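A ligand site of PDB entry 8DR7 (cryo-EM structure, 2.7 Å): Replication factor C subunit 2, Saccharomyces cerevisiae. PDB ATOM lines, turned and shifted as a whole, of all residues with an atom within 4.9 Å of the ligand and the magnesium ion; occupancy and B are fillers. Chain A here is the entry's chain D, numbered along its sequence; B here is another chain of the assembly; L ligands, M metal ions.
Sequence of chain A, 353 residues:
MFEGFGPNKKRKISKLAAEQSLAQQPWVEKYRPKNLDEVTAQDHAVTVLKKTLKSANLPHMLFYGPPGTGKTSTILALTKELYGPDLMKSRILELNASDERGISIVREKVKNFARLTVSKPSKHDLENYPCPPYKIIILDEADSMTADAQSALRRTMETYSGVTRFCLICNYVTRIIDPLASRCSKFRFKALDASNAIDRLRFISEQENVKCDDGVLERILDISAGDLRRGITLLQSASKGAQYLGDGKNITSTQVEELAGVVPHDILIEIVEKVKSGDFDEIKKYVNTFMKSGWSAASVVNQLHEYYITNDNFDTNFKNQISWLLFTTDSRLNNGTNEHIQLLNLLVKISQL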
ATOM      1  N   TRP A  27      -0.698 -31.784  12.742  1.00  0.00           N
ATOM      2  CA  TRP A  27      -1.391 -31.204  11.592  1.00  0.00           C
ATOM      3  C   TRP A  27      -0.608 -30.049  10.990  1.00  0.00           C
ATOM      4  O   TRP A  27      -0.660 -29.822   9.775  1.00  0.00           O
ATOM      5  CB  TRP A  27      -2.794 -30.732  11.998  1.00  0.00           C
ATOM      6  CG  TRP A  27      -3.737 -31.850  12.325  1.00  0.00           C
ATOM      7  CD1 TRP A  27      -3.426 -33.177  12.469  1.00  0.00           C
ATOM      8  CD2 TRP A  27      -5.149 -31.743  12.538  1.00  0.00           C
ATOM      9  NE1 TRP A  27      -4.558 -33.894  12.765  1.00  0.00           N
ATOM     10  CE2 TRP A  27      -5.631 -33.036  12.810  1.00  0.00           C
ATOM     11  CE3 TRP A  27      -6.047 -30.680  12.520  1.00  0.00           C
ATOM     12  CZ2 TRP A  27      -6.968 -33.299  13.064  1.00  0.00           C
ATOM     13  CZ3 TRP A  27      -7.385 -30.934  12.778  1.00  0.00           C
ATOM     14  CH2 TRP A  27      -7.837 -32.233  13.044  1.00  0.00           C
ATOM     15  N   VAL A  28       0.137 -29.302  11.812  1.00  0.00           N
ATOM     16  CA  VAL A  28       0.929 -28.193  11.287  1.00  0.00           C
ATOM     17  C   VAL A  28       2.007 -28.713  10.354  1.00  0.00           C
ATOM     18  O   VAL A  28       2.283 -28.101   9.304  1.00  0.00           O
ATOM     19  CB  VAL A  28       1.521 -27.354  12.439  1.00  0.00           C
ATOM     20  CG1 VAL A  28       0.416 -26.663  13.220  1.00  0.00           C
ATOM     21  CG2 VAL A  28       2.366 -28.220  13.365  1.00  0.00           C
ATOM     22  N   GLU A  29       2.637 -29.831  10.700  1.00  0.00           N
ATOM     23  CA  GLU A  29       3.637 -30.441   9.829  1.00  0.00           C
ATOM     24  C   GLU A  29       3.015 -31.325   8.747  1.00  0.00           C
ATOM     25  O   GLU A  29       3.547 -31.394   7.634  1.00  0.00           O
ATOM     26  CB  GLU A  29       4.624 -31.279  10.649  1.00  0.00           C
ATOM     27  CG  GLU A  29       5.167 -30.587  11.883  1.00  0.00           C
ATOM     28  CD  GLU A  29       6.173 -29.497  11.554  1.00  0.00           C
ATOM     29  OE1 GLU A  29       6.583 -28.760  12.482  1.00  0.00           O
ATOM     30  OE2 GLU A  29       6.548 -29.370  10.368  1.00  0.00           O
ATOM     31  N   TYR A  31       0.206 -30.902   7.107  1.00  0.00           N
ATOM     32  CA  TYR A  31      -0.340 -30.060   6.048  1.00  0.00           C
ATOM     33  C   TYR A  31       0.608 -28.935   5.654  1.00  0.00           C
ATOM     34  O   TYR A  31       0.150 -27.902   5.143  1.00  0.00           O
ATOM     35  CB  TYR A  31      -1.702 -29.495   6.481  1.00  0.00           C
ATOM     36  CG  TYR A  31      -2.776 -30.550   6.569  1.00  0.00           C
ATOM     37  CD1 TYR A  31      -3.396 -31.042   5.440  1.00  0.00           C
ATOM     38  CD2 TYR A  31      -3.164 -31.063   7.809  1.00  0.00           C
ATOM     39  CE1 TYR A  31      -4.370 -32.008   5.511  1.00  0.00           C
ATOM     40  CE2 TYR A  31      -4.148 -32.027   7.894  1.00  0.00           C
ATOM     41  CZ  TYR A  31      -4.751 -32.501   6.738  1.00  0.00           C
ATOM     42  OH  TYR A  31      -5.726 -33.458   6.814  1.00  0.00           O
ATOM     43  N   ARG A  32       1.900 -29.113   5.870  1.00  0.00           N
ATOM     44  CA  ARG A  32       2.860 -28.122   5.407  1.00  0.00           C
ATOM     45  C   ARG A  32       2.854 -28.085   3.873  1.00  0.00           C
ATOM     46  O   ARG A  32       2.818 -29.138   3.227  1.00  0.00           O
ATOM     47  CB  ARG A  32       4.267 -28.455   5.914  1.00  0.00           C
ATOM     48  CG  ARG A  32       5.374 -27.569   5.335  1.00  0.00           C
ATOM     49  CD  ARG A  32       6.729 -27.961   5.895  1.00  0.00           C
ATOM     50  NE  ARG A  32       6.848 -27.624   7.310  1.00  0.00           N
ATOM     51  CZ  ARG A  32       7.139 -26.420   7.780  1.00  0.00           C
ATOM     52  NH1 ARG A  32       7.341 -25.399   6.971  1.00  0.00           N
ATOM     53  NH2 ARG A  32       7.219 -26.237   9.096  1.00  0.00           N
ATOM     54  N   PRO A  33       2.886 -26.895   3.267  1.00  0.00           N
ATOM     55  CA  PRO A  33       2.870 -26.828   1.799  1.00  0.00           C
ATOM     56  C   PRO A  33       4.035 -27.608   1.192  1.00  0.00           C
ATOM     57  O   PRO A  33       5.158 -27.580   1.704  1.00  0.00           O
ATOM     58  CB  PRO A  33       2.975 -25.331   1.507  1.00  0.00           C
ATOM     59  CG  PRO A  33       2.411 -24.678   2.714  1.00  0.00           C
ATOM     60  CD  PRO A  33       2.776 -25.556   3.866  1.00  0.00           C
ATOM     61  N   GLU A  38       0.132 -24.155  -3.085  1.00  0.00           N
ATOM     62  CA  GLU A  38      -0.593 -24.264  -1.821  1.00  0.00           C
ATOM     63  C   GLU A  38      -0.444 -23.037  -0.945  1.00  0.00           C
ATOM     64  O   GLU A  38      -1.090 -22.967   0.111  1.00  0.00           O
ATOM     65  CB  GLU A  38      -0.128 -25.506  -1.061  1.00  0.00           C
ATOM     66  CG  GLU A  38       0.231 -26.686  -1.948  1.00  0.00           C
ATOM     67  CD  GLU A  38      -0.053 -28.026  -1.283  1.00  0.00           C
ATOM     68  OE1 GLU A  38       0.913 -28.752  -0.979  1.00  0.00           O
ATOM     69  OE2 GLU A  38      -1.235 -28.345  -1.070  1.00  0.00           O
ATOM     70  N   VAL A  39       0.371 -22.067  -1.334  1.00  0.00           N
ATOM     71  CA  VAL A  39       0.489 -20.813  -0.602  1.00  0.00           C
ATOM     72  C   VAL A  39      -0.750 -19.975  -0.876  1.00  0.00           C
ATOM     73  O   VAL A  39      -1.155 -19.800  -2.033  1.00  0.00           O
ATOM     74  CB  VAL A  39       1.774 -20.071  -0.996  1.00  0.00           C
ATOM     75  CG1 VAL A  39       1.900 -18.772  -0.203  1.00  0.00           C
ATOM     76  CG2 VAL A  39       2.996 -20.956  -0.783  1.00  0.00           C
ATOM     77  N   THR A  40      -1.358 -19.445   0.180  1.00  0.00           N
ATOM     78  CA  THR A  40      -2.683 -18.842   0.070  1.00  0.00           C
ATOM     79  C   THR A  40      -2.627 -17.331  -0.173  1.00  0.00           C
ATOM     80  O   THR A  40      -3.120 -16.856  -1.199  1.00  0.00           O
ATOM     81  CB  THR A  40      -3.488 -19.133   1.352  1.00  0.00           C
ATOM     82  OG1 THR A  40      -2.611 -19.123   2.480  1.00  0.00           O
ATOM     83  CG2 THR A  40      -4.186 -20.479   1.256  1.00  0.00           C
ATOM     84  N   GLN A  42       0.146 -15.128  -0.149  1.00  0.00           N
ATOM     85  CA  GLN A  42       1.443 -14.556  -0.493  1.00  0.00           C
ATOM     86  C   GLN A  42       1.657 -14.587  -2.001  1.00  0.00           C
ATOM     87  O   GLN A  42       2.744 -14.893  -2.491  1.00  0.00           O
ATOM     88  CB  GLN A  42       2.575 -15.297   0.226  1.00  0.00           C
ATOM     89  CG  GLN A  42       2.255 -15.701   1.663  1.00  0.00           C
ATOM     90  CD  GLN A  42       2.219 -14.503   2.602  1.00  0.00           C
ATOM     91  OE1 GLN A  42       2.441 -13.372   2.195  1.00  0.00           O
ATOM     92  NE2 GLN A  42       1.926 -14.768   3.873  1.00  0.00           N
ATOM     93  N   GLY A  65       8.571 -11.018   7.749  1.00  0.00           N
ATOM     94  CA  GLY A  65       7.172 -10.956   8.098  1.00  0.00           C
ATOM     95  C   GLY A  65       6.904 -11.482   9.491  1.00  0.00           C
ATOM     96  O   GLY A  65       7.820 -11.933  10.187  1.00  0.00           O
ATOM     97  N   PRO A  66       5.653 -11.446   9.922  1.00  0.00           N
ATOM     98  CA  PRO A  66       5.308 -11.935  11.265  1.00  0.00           C
ATOM     99  C   PRO A  66       5.404 -13.447  11.336  1.00  0.00           C
ATOM    100  O   PRO A  66       5.426 -14.128  10.296  1.00  0.00           O
ATOM    101  CB  PRO A  66       3.862 -11.447  11.463  1.00  0.00           C
ATOM    102  CG  PRO A  66       3.325 -11.278  10.085  1.00  0.00           C
ATOM    103  CD  PRO A  66       4.475 -10.917   9.199  1.00  0.00           C
ATOM    104  N   PRO A  67       5.464 -14.015  12.535  1.00  0.00           N
ATOM    105  CA  PRO A  67       5.607 -15.472  12.657  1.00  0.00           C
ATOM    106  C   PRO A  67       4.409 -16.206  12.063  1.00  0.00           C
ATOM    107  O   PRO A  67       3.282 -15.706  12.053  1.00  0.00           O
ATOM    108  CB  PRO A  67       5.705 -15.700  14.171  1.00  0.00           C
ATOM    109  CG  PRO A  67       6.141 -14.397  14.729  1.00  0.00           C
ATOM    110  CD  PRO A  67       5.510 -13.353  13.848  1.00  0.00           C
ATOM    111  N   GLY A  68       4.671 -17.410  11.571  1.00  0.00           N
ATOM    112  CA  GLY A  68       3.612 -18.270  11.049  1.00  0.00           C
ATOM    113  C   GLY A  68       2.941 -17.756   9.799  1.00  0.00           C
ATOM    114  O   GLY A  68       1.712 -17.814   9.692  1.00  0.00           O
ATOM    115  N   THR A  69       3.718 -17.250   8.835  1.00  0.00           N
ATOM    116  CA  THR A  69       3.171 -16.766   7.575  1.00  0.00           C
ATOM    117  C   THR A  69       3.540 -17.645   6.386  1.00  0.00           C
ATOM    118  O   THR A  69       2.950 -17.489   5.311  1.00  0.00           O
ATOM    119  CB  THR A  69       3.658 -15.332   7.304  1.00  0.00           C
ATOM    120  OG1 THR A  69       5.070 -15.251   7.495  1.00  0.00           O
ATOM    121  CG2 THR A  69       2.951 -14.356   8.229  1.00  0.00           C
ATOM    122  N   GLY A  70       4.490 -18.565   6.542  1.00  0.00           N
ATOM    123  CA  GLY A  70       4.840 -19.483   5.473  1.00  0.00           C
ATOM    124  C   GLY A  70       6.048 -19.059   4.665  1.00  0.00           C
ATOM    125  O   GLY A  70       6.016 -19.104   3.437  1.00  0.00           O
ATOM    126  N   LYS A  71       7.115 -18.644   5.343  1.00  0.00           N
ATOM    127  CA  LYS A  71       8.344 -18.251   4.666  1.00  0.00           C
ATOM    128  C   LYS A  71       9.264 -19.449   4.426  1.00  0.00           C
ATOM    129  O   LYS A  71       9.696 -19.703   3.297  1.00  0.00           O
ATOM    130  CB  LYS A  71       9.083 -17.184   5.480  1.00  0.00           C
ATOM    131  CG  LYS A  71       8.241 -15.942   5.772  1.00  0.00           C
ATOM    132  CD  LYS A  71       9.020 -14.894   6.547  1.00  0.00           C
ATOM    133  CE  LYS A  71       9.308 -15.324   7.975  1.00  0.00           C
ATOM    134  NZ  LYS A  71       8.064 -15.529   8.766  1.00  0.00           N
ATOM    135  N   THR A  72       9.579 -20.195   5.488  1.00  0.00           N
ATOM    136  CA  THR A  72      10.393 -21.401   5.326  1.00  0.00           C
ATOM    137  C   THR A  72       9.695 -22.417   4.432  1.00  0.00           C
ATOM    138  O   THR A  72      10.337 -23.050   3.591  1.00  0.00           O
ATOM    139  CB  THR A  72      10.718 -22.012   6.689  1.00  0.00           C
ATOM    140  OG1 THR A  72      11.547 -23.170   6.507  1.00  0.00           O
ATOM    141  CG2 THR A  72       9.454 -22.426   7.417  1.00  0.00           C
ATOM    142  N   SER A  73       8.380 -22.566   4.598  1.00  0.00           N
ATOM    143  CA  SER A  73       7.628 -23.453   3.717  1.00  0.00           C
ATOM    144  C   SER A  73       7.727 -22.978   2.268  1.00  0.00           C
ATOM    145  O   SER A  73       7.901 -23.793   1.352  1.00  0.00           O
ATOM    146  CB  SER A  73       6.169 -23.528   4.167  1.00  0.00           C
ATOM    147  OG  SER A  73       6.076 -23.931   5.518  1.00  0.00           O
ATOM    148  N   ASP A 140      18.236 -19.166   7.452  1.00  0.00           N
ATOM    149  CA  ASP A 140      17.035 -18.952   8.253  1.00  0.00           C
ATOM    150  C   ASP A 140      17.387 -18.311   9.586  1.00  0.00           C
ATOM    151  O   ASP A 140      18.493 -18.480  10.111  1.00  0.00           O
ATOM    152  CB  ASP A 140      16.312 -20.281   8.475  1.00  0.00           C
ATOM    153  CG  ASP A 140      14.820 -20.107   8.644  1.00  0.00           C
ATOM    154  OD1 ASP A 140      14.376 -18.985   8.957  1.00  0.00           O
ATOM    155  OD2 ASP A 140      14.076 -21.094   8.452  1.00  0.00           O
ATOM    156  N   GLU A 141      16.424 -17.563  10.137  1.00  0.00           N
ATOM    157  CA  GLU A 141      16.622 -16.844  11.395  1.00  0.00           C
ATOM    158  C   GLU A 141      17.845 -15.945  11.313  1.00  0.00           C
ATOM    159  O   GLU A 141      18.661 -15.853  12.239  1.00  0.00           O
ATOM    160  CB  GLU A 141      16.738 -17.829  12.573  1.00  0.00           C
ATOM    161  CG  GLU A 141      15.404 -18.214  13.186  1.00  0.00           C
ATOM    162  CD  GLU A 141      14.932 -19.589  12.741  1.00  0.00           C
ATOM    163  OE1 GLU A 141      15.754 -20.526  12.715  1.00  0.00           O
ATOM    164  OE2 GLU A 141      13.731 -19.730  12.406  1.00  0.00           O
ATOM    165  N   ASN A 171      12.363 -12.406  11.000  1.00  0.00           N
ATOM    166  CA  ASN A 171      11.110 -11.867  11.509  1.00  0.00           C
ATOM    167  C   ASN A 171      11.152 -10.368  11.729  1.00  0.00           C
ATOM    168  O   ASN A 171      10.129  -9.692  11.577  1.00  0.00           O
ATOM    169  CB  ASN A 171      10.735 -12.551  12.821  1.00  0.00           C
ATOM    170  CG  ASN A 171      10.008 -13.869  12.616  1.00  0.00           C
ATOM    171  OD1 ASN A 171      10.436 -14.906  13.129  1.00  0.00           O
ATOM    172  ND2 ASN A 171       8.904 -13.827  11.875  1.00  0.00           N
ATOM    173  N   LEU A 192      -2.021 -13.539   8.047  1.00  0.00           N
ATOM    174  CA  LEU A 192      -3.049 -14.463   7.576  1.00  0.00           C
ATOM    175  C   LEU A 192      -4.278 -14.309   8.473  1.00  0.00           C
ATOM    176  O   LEU A 192      -4.312 -14.805   9.598  1.00  0.00           O
ATOM    177  CB  LEU A 192      -2.532 -15.900   7.582  1.00  0.00           C
ATOM    178  CG  LEU A 192      -1.300 -16.155   6.718  1.00  0.00           C
ATOM    179  CD1 LEU A 192      -0.825 -17.591   6.870  1.00  0.00           C
ATOM    180  CD2 LEU A 192      -1.596 -15.845   5.254  1.00  0.00           C
ATOM    181  N   ARG A 200      -7.747 -22.292   3.327  1.00  0.00           N
ATOM    182  CA  ARG A 200      -6.836 -23.358   3.740  1.00  0.00           C
ATOM    183  C   ARG A 200      -7.344 -24.049   5.006  1.00  0.00           C
ATOM    184  O   ARG A 200      -7.309 -25.284   5.097  1.00  0.00           O
ATOM    185  CB  ARG A 200      -5.437 -22.794   3.964  1.00  0.00           C
ATOM    186  CG  ARG A 200      -4.373 -23.843   4.274  1.00  0.00           C
ATOM    187  CD  ARG A 200      -4.102 -24.751   3.080  1.00  0.00           C
ATOM    188  NE  ARG A 200      -3.121 -25.783   3.388  1.00  0.00           N
ATOM    189  CZ  ARG A 200      -2.718 -26.713   2.539  1.00  0.00           C
ATOM    190  NH1 ARG A 200      -3.191 -26.773   1.297  1.00  0.00           N
ATOM    191  NH2 ARG A 200      -1.818 -27.611   2.924  1.00  0.00           N
ATOM    192  N   LEU A 228      -1.258 -18.730  11.172  1.00  0.00           N
ATOM    193  CA  LEU A 228      -1.993 -19.908  10.736  1.00  0.00           C
ATOM    194  C   LEU A 228      -1.566 -21.160  11.506  1.00  0.00           C
ATOM    195  O   LEU A 228      -2.369 -22.079  11.678  1.00  0.00           O
ATOM    196  CB  LEU A 228      -1.798 -20.123   9.238  1.00  0.00           C
ATOM    197  CG  LEU A 228      -2.777 -21.063   8.530  1.00  0.00           C
ATOM    198  CD1 LEU A 228      -4.225 -20.691   8.823  1.00  0.00           C
ATOM    199  CD2 LEU A 228      -2.528 -21.045   7.024  1.00  0.00           C
ATOM    200  N   ARG A 229      -0.317 -21.200  11.973  1.00  0.00           N
ATOM    201  CA  ARG A 229       0.119 -22.340  12.774  1.00  0.00           C
ATOM    202  C   ARG A 229      -0.686 -22.447  14.061  1.00  0.00           C
ATOM    203  O   ARG A 229      -1.124 -23.546  14.444  1.00  0.00           O
ATOM    204  CB  ARG A 229       1.614 -22.219  13.085  1.00  0.00           C
ATOM    205  CG  ARG A 229       2.297 -23.542  13.408  1.00  0.00           C
ATOM    206  CD  ARG A 229       3.567 -23.341  14.215  1.00  0.00           C
ATOM    207  NE  ARG A 229       4.737 -23.130  13.366  1.00  0.00           N
ATOM    208  CZ  ARG A 229       5.306 -21.953  13.143  1.00  0.00           C
ATOM    209  NH1 ARG A 229       4.845 -20.834  13.690  1.00  0.00           N
ATOM    210  NH2 ARG A 229       6.374 -21.889  12.348  1.00  0.00           N
ATOM    211  N   ILE A 232      -4.173 -23.721  13.238  1.00  0.00           N
ATOM    212  CA  ILE A 232      -4.176 -25.148  12.963  1.00  0.00           C
ATOM    213  C   ILE A 232      -4.045 -25.947  14.261  1.00  0.00           C
ATOM    214  O   ILE A 232      -4.714 -26.970  14.448  1.00  0.00           O
ATOM    215  CB  ILE A 232      -3.059 -25.518  11.962  1.00  0.00           C
ATOM    216  CG1 ILE A 232      -3.364 -24.913  10.593  1.00  0.00           C
ATOM    217  CG2 ILE A 232      -2.912 -27.028  11.864  1.00  0.00           C
ATOM    218  CD1 ILE A 232      -2.147 -24.789   9.699  1.00  0.00           C
ATOM    219  N   ARG B 155      13.704 -23.105  17.632  1.00  0.00           N
ATOM    220  CA  ARG B 155      12.647 -22.873  16.659  1.00  0.00           C
ATOM    221  C   ARG B 155      12.650 -23.944  15.565  1.00  0.00           C
ATOM    222  O   ARG B 155      11.604 -24.541  15.268  1.00  0.00           O
ATOM    223  CB  ARG B 155      12.787 -21.484  16.029  1.00  0.00           C
ATOM    224  CG  ARG B 155      12.415 -20.345  16.963  1.00  0.00           C
ATOM    225  CD  ARG B 155      12.731 -19.001  16.332  1.00  0.00           C
ATOM    226  NE  ARG B 155      12.036 -18.808  15.069  1.00  0.00           N
ATOM    227  CZ  ARG B 155      12.082 -17.707  14.339  1.00  0.00           C
ATOM    228  NH1 ARG B 155      12.799 -16.656  14.712  1.00  0.00           N
ATOM    229  NH2 ARG B 155      11.409 -17.652  13.190  1.00  0.00           N
ATOM    230  N   ARG B 156      13.806 -24.202  14.966  1.00  0.00           N
ATOM    231  CA  ARG B 156      13.883 -25.200  13.895  1.00  0.00           C
ATOM    232  C   ARG B 156      13.994 -26.622  14.439  1.00  0.00           C
ATOM    233  O   ARG B 156      13.602 -27.576  13.756  1.00  0.00           O
ATOM    234  CB  ARG B 156      15.069 -24.901  12.980  1.00  0.00           C
ATOM    235  CG  ARG B 156      14.854 -23.745  12.009  1.00  0.00           C
ATOM    236  CD  ARG B 156      13.710 -23.995  11.029  1.00  0.00           C
ATOM    237  NE  ARG B 156      13.934 -25.188  10.222  1.00  0.00           N
ATOM    238  CZ  ARG B 156      13.018 -25.740   9.443  1.00  0.00           C
ATOM    239  NH1 ARG B 156      11.797 -25.253   9.344  1.00  0.00           N
ATOM    240  NH2 ARG B 156      13.336 -26.827   8.746  1.00  0.00           N
ATOM    241  N   GLU B 159      10.762 -28.333  14.799  1.00  0.00           N
ATOM    242  CA  GLU B 159      10.057 -28.503  13.532  1.00  0.00           C
ATOM    243  C   GLU B 159      10.641 -29.605  12.664  1.00  0.00           C
ATOM    244  O   GLU B 159       9.890 -30.427  12.138  1.00  0.00           O
ATOM    245  CB  GLU B 159      10.065 -27.175  12.753  1.00  0.00           C
ATOM    246  CG  GLU B 159       8.979 -26.201  13.185  1.00  0.00           C
ATOM    247  CD  GLU B 159       8.531 -25.280  12.067  1.00  0.00           C
ATOM    248  OE1 GLU B 159       9.407 -24.717  11.371  1.00  0.00           O
ATOM    249  OE2 GLU B 159       7.313 -25.124  11.877  1.00  0.00           O
ATOM    250  N   PRO B 180       7.759 -16.828  18.268  1.00  0.00           N
ATOM    251  CA  PRO B 180       7.881 -18.084  17.494  1.00  0.00           C
ATOM    252  C   PRO B 180       7.706 -19.330  18.330  1.00  0.00           C
ATOM    253  O   PRO B 180       7.097 -20.300  17.875  1.00  0.00           O
ATOM    254  CB  PRO B 180       9.300 -17.981  16.914  1.00  0.00           C
ATOM    255  CG  PRO B 180       9.583 -16.519  16.860  1.00  0.00           C
ATOM    256  CD  PRO B 180       8.919 -15.949  18.076  1.00  0.00           C
ATOM    257  N   ARG B 184       4.749 -22.286  17.974  1.00  0.00           N
ATOM    258  CA  ARG B 184       5.087 -23.686  17.720  1.00  0.00           C
ATOM    259  C   ARG B 184       4.599 -24.627  18.822  1.00  0.00           C
ATOM    260  O   ARG B 184       4.811 -25.835  18.698  1.00  0.00           O
ATOM    261  CB  ARG B 184       6.607 -23.831  17.565  1.00  0.00           C
ATOM    262  CG  ARG B 184       7.158 -23.269  16.264  1.00  0.00           C
ATOM    263  CD  ARG B 184       8.672 -23.299  16.248  1.00  0.00           C
ATOM    264  NE  ARG B 184       9.221 -23.091  14.912  1.00  0.00           N
ATOM    265  CZ  ARG B 184       9.367 -21.897  14.353  1.00  0.00           C
ATOM    266  NH1 ARG B 184       9.021 -20.780  14.978  1.00  0.00           N
ATOM    267  NH2 ARG B 184       9.886 -21.818  13.131  1.00  0.00           N
HETATM  268  P1  LIG L   1       8.470 -18.134  11.518  1.00  0.00           P
HETATM  269  S1  LIG L   1       8.356 -18.255  13.426  1.00  0.00           S
HETATM  270  O1  LIG L   1       9.817 -18.971  10.973  1.00  0.00           O
HETATM  271  O2  LIG L   1       8.614 -16.516  11.071  1.00  0.00           O
HETATM  272  P2  LIG L   1       6.975 -19.182   9.253  1.00  0.00           P
HETATM  273  O3  LIG L   1       6.815 -17.910   8.426  1.00  0.00           O
HETATM  274  O4  LIG L   1       8.215 -19.921   8.802  1.00  0.00           O
HETATM  275  O5  LIG L   1       7.119 -18.794  10.858  1.00  0.00           O
HETATM  276  P3  LIG L   1       5.761 -21.730   8.809  1.00  0.00           P
HETATM  277  O6  LIG L   1       6.446 -21.988   7.507  1.00  0.00           O
HETATM  278  O7  LIG L   1       6.560 -22.361   9.939  1.00  0.00           O
HETATM  279  O8  LIG L   1       5.663 -20.140   9.053  1.00  0.00           O
HETATM  280  O9  LIG L   1       4.234 -22.402   8.783  1.00  0.00           O
HETATM  281  C1  LIG L   1       3.887 -23.301   9.777  1.00  0.00           C
HETATM  282  C2  LIG L   1       2.627 -24.013   9.390  1.00  0.00           C
HETATM  283  O10 LIG L   1       1.629 -23.162   9.339  1.00  0.00           O
HETATM  284  C3  LIG L   1       2.800 -24.662   7.871  1.00  0.00           C
HETATM  285  O11 LIG L   1       3.269 -26.076   7.967  1.00  0.00           O
HETATM  286  C4  LIG L   1       1.678 -24.617   7.356  1.00  0.00           C
HETATM  287  O12 LIG L   1       0.901 -25.843   7.728  1.00  0.00           O
HETATM  288  C5  LIG L   1       0.989 -23.317   7.980  1.00  0.00           C
HETATM  289  N1  LIG L   1       1.228 -22.226   7.254  1.00  0.00           N
HETATM  290  C6  LIG L   1       1.909 -21.116   7.469  1.00  0.00           C
HETATM  291  N2  LIG L   1       1.813 -20.349   6.381  1.00  0.00           N
HETATM  292  C7  LIG L   1       1.052 -20.997   5.491  1.00  0.00           C
HETATM  293  C8  LIG L   1       0.633 -20.670   4.216  1.00  0.00           C
HETATM  294  N3  LIG L   1       0.946 -19.431   3.488  1.00  0.00           N
HETATM  295  N4  LIG L   1      -0.124 -21.507   3.541  1.00  0.00           N
HETATM  296  C9  LIG L   1      -0.494 -22.680   4.094  1.00  0.00           C
HETATM  297  N5  LIG L   1      -0.088 -22.997   5.330  1.00  0.00           N
HETATM  298  C10 LIG L   1       0.690 -22.159   6.026  1.00  0.00           C
HETATM  299 MG    MG M   1       9.884 -21.118   9.921  1.00  0.00          MG
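The guanidinium group (NH2) of Arg 32 is in salt-bridge range of the side-chain carboxylate (OE2) of Glu 29 (3.4 Å). The guanidinium group of Arg 200 lies within hydrogen-bond range of the backbone carbonyl oxygen of Tyr 31 (3.0 Å). The backbone carbonyl oxygen (O) of Pro 66 is in hydrogen-bond range of the side-chain hydroxyl (OG1) of Thr 69. O of Arg 155 of chain B is in hydrogen-bond range of NE of Arg 184 of chain B (2.8 Å). The side-chain amino group (NZ) of Lys 71 is in hydrogen-bond range of the side-chain hydroxyl (OG1) of Thr 69 (3.3 Å). The guanidinium group of Arg 155 of chain B lies within salt-bridge range of the side-chain carboxylate of Glu 141. OG of Ser 73 sits at hydrogen-bond distance from NH1 of Arg 32 (2.4 Å). The side-chain amide nitrogen of Gln 42 sits at hydrogen-bond distance from the backbone carbonyl oxygen of Thr 69.
Thr 72 touches the magnesium ion (CG2 to MG, 2.9 Å). Glu 159 of chain B touches the magnesium ion. NH2 of Arg 184 of chain B touches the magnesium ion, at 3.3 Å. The nearest printed residue that does not touch the magnesium ion is Arg 229 (4.3 Å).
O7 of the ligand sits close to OE2 of Glu 159 of chain B, 3.5 Å away. Pro 33 touches the ligand. O of Glu 38 touches N4 of the ligand, at 3.9 Å. Val 39 touches the ligand (CG1 to N3, 3.9 Å). OG1 of Thr 40 touches N4 of the ligand, at 3.6 Å. CA of Pro 67 touches O2 of the ligand, 3.6 Å away. Thr 72 touches the ligand (CG2 to O6, 3.0 Å). CD1 of Leu 192 touches N2 of the ligand, 3.8 Å away. Leu 228 touches the ligand. CD1 of Ile 232 touches O12 of the ligand, at 3.8 Å. Pro 180 of chain B touches the ligand (CB to S1, 3.6 Å). Of the 32 residues printed, 23 come within 4 Å of the ligand.
The guanidinium group of Arg 32 lies within salt-bridge range of an oxygen (O6) of the ligand (3.6 Å). O5 of the ligand sits at hydrogen-bond distance from N of Gly 68 (2.9 Å). The backbone NH of Lys 71 lies within hydrogen-bond range of an oxygen (O3) of the ligand. A sulfur (S1) of the ligand sits close to the guanidinium group (NH1) of Arg 184 of chain B, 3.0 Å away. A sulfur (S1) of the ligand sits close to the guanidinium group of Arg 155 of chain B (3.1 Å). An oxygen (O11) of the ligand lies within hydrogen-bond range of the backbone carbonyl oxygen (O) of Val 28. O3 of the ligand lies within hydrogen-bond range of OG1 of Thr 69 (3.3 Å). An oxygen (O6) of the ligand lies within hydrogen-bond range of the side-chain hydroxyl (OG) of Ser 73, 2.8 Å away. The side-chain amide nitrogen (ND2) of Asn 171 sits at hydrogen-bond distance from an oxygen (O2) of the ligand, 2.8 Å away. O of Tyr 31 lies within hydrogen-bond range of O12 of the ligand. The side-chain amino group (NZ) of Lys 71 lies within salt-bridge range of an oxygen (O3) of the ligand, 2.7 Å away. The guanidinium group (NH2) of Arg 229 lies within salt-bridge range of an oxygen (O7) of the ligand (2.5 Å). O3 of the ligand is in hydrogen-bond range of N of Gly 70 (3.1 Å). O3 of the ligand lies within hydrogen-bond range of N of Thr 69 (3.2 Å). O of Thr 69 is in hydrogen-bond range of N3 of the ligand, at 3.3 Å.
O4 of the ligand binds the magnesium ion (2.3 Å). The magnesium ion is bound by O1 of the ligand (2.4 Å).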
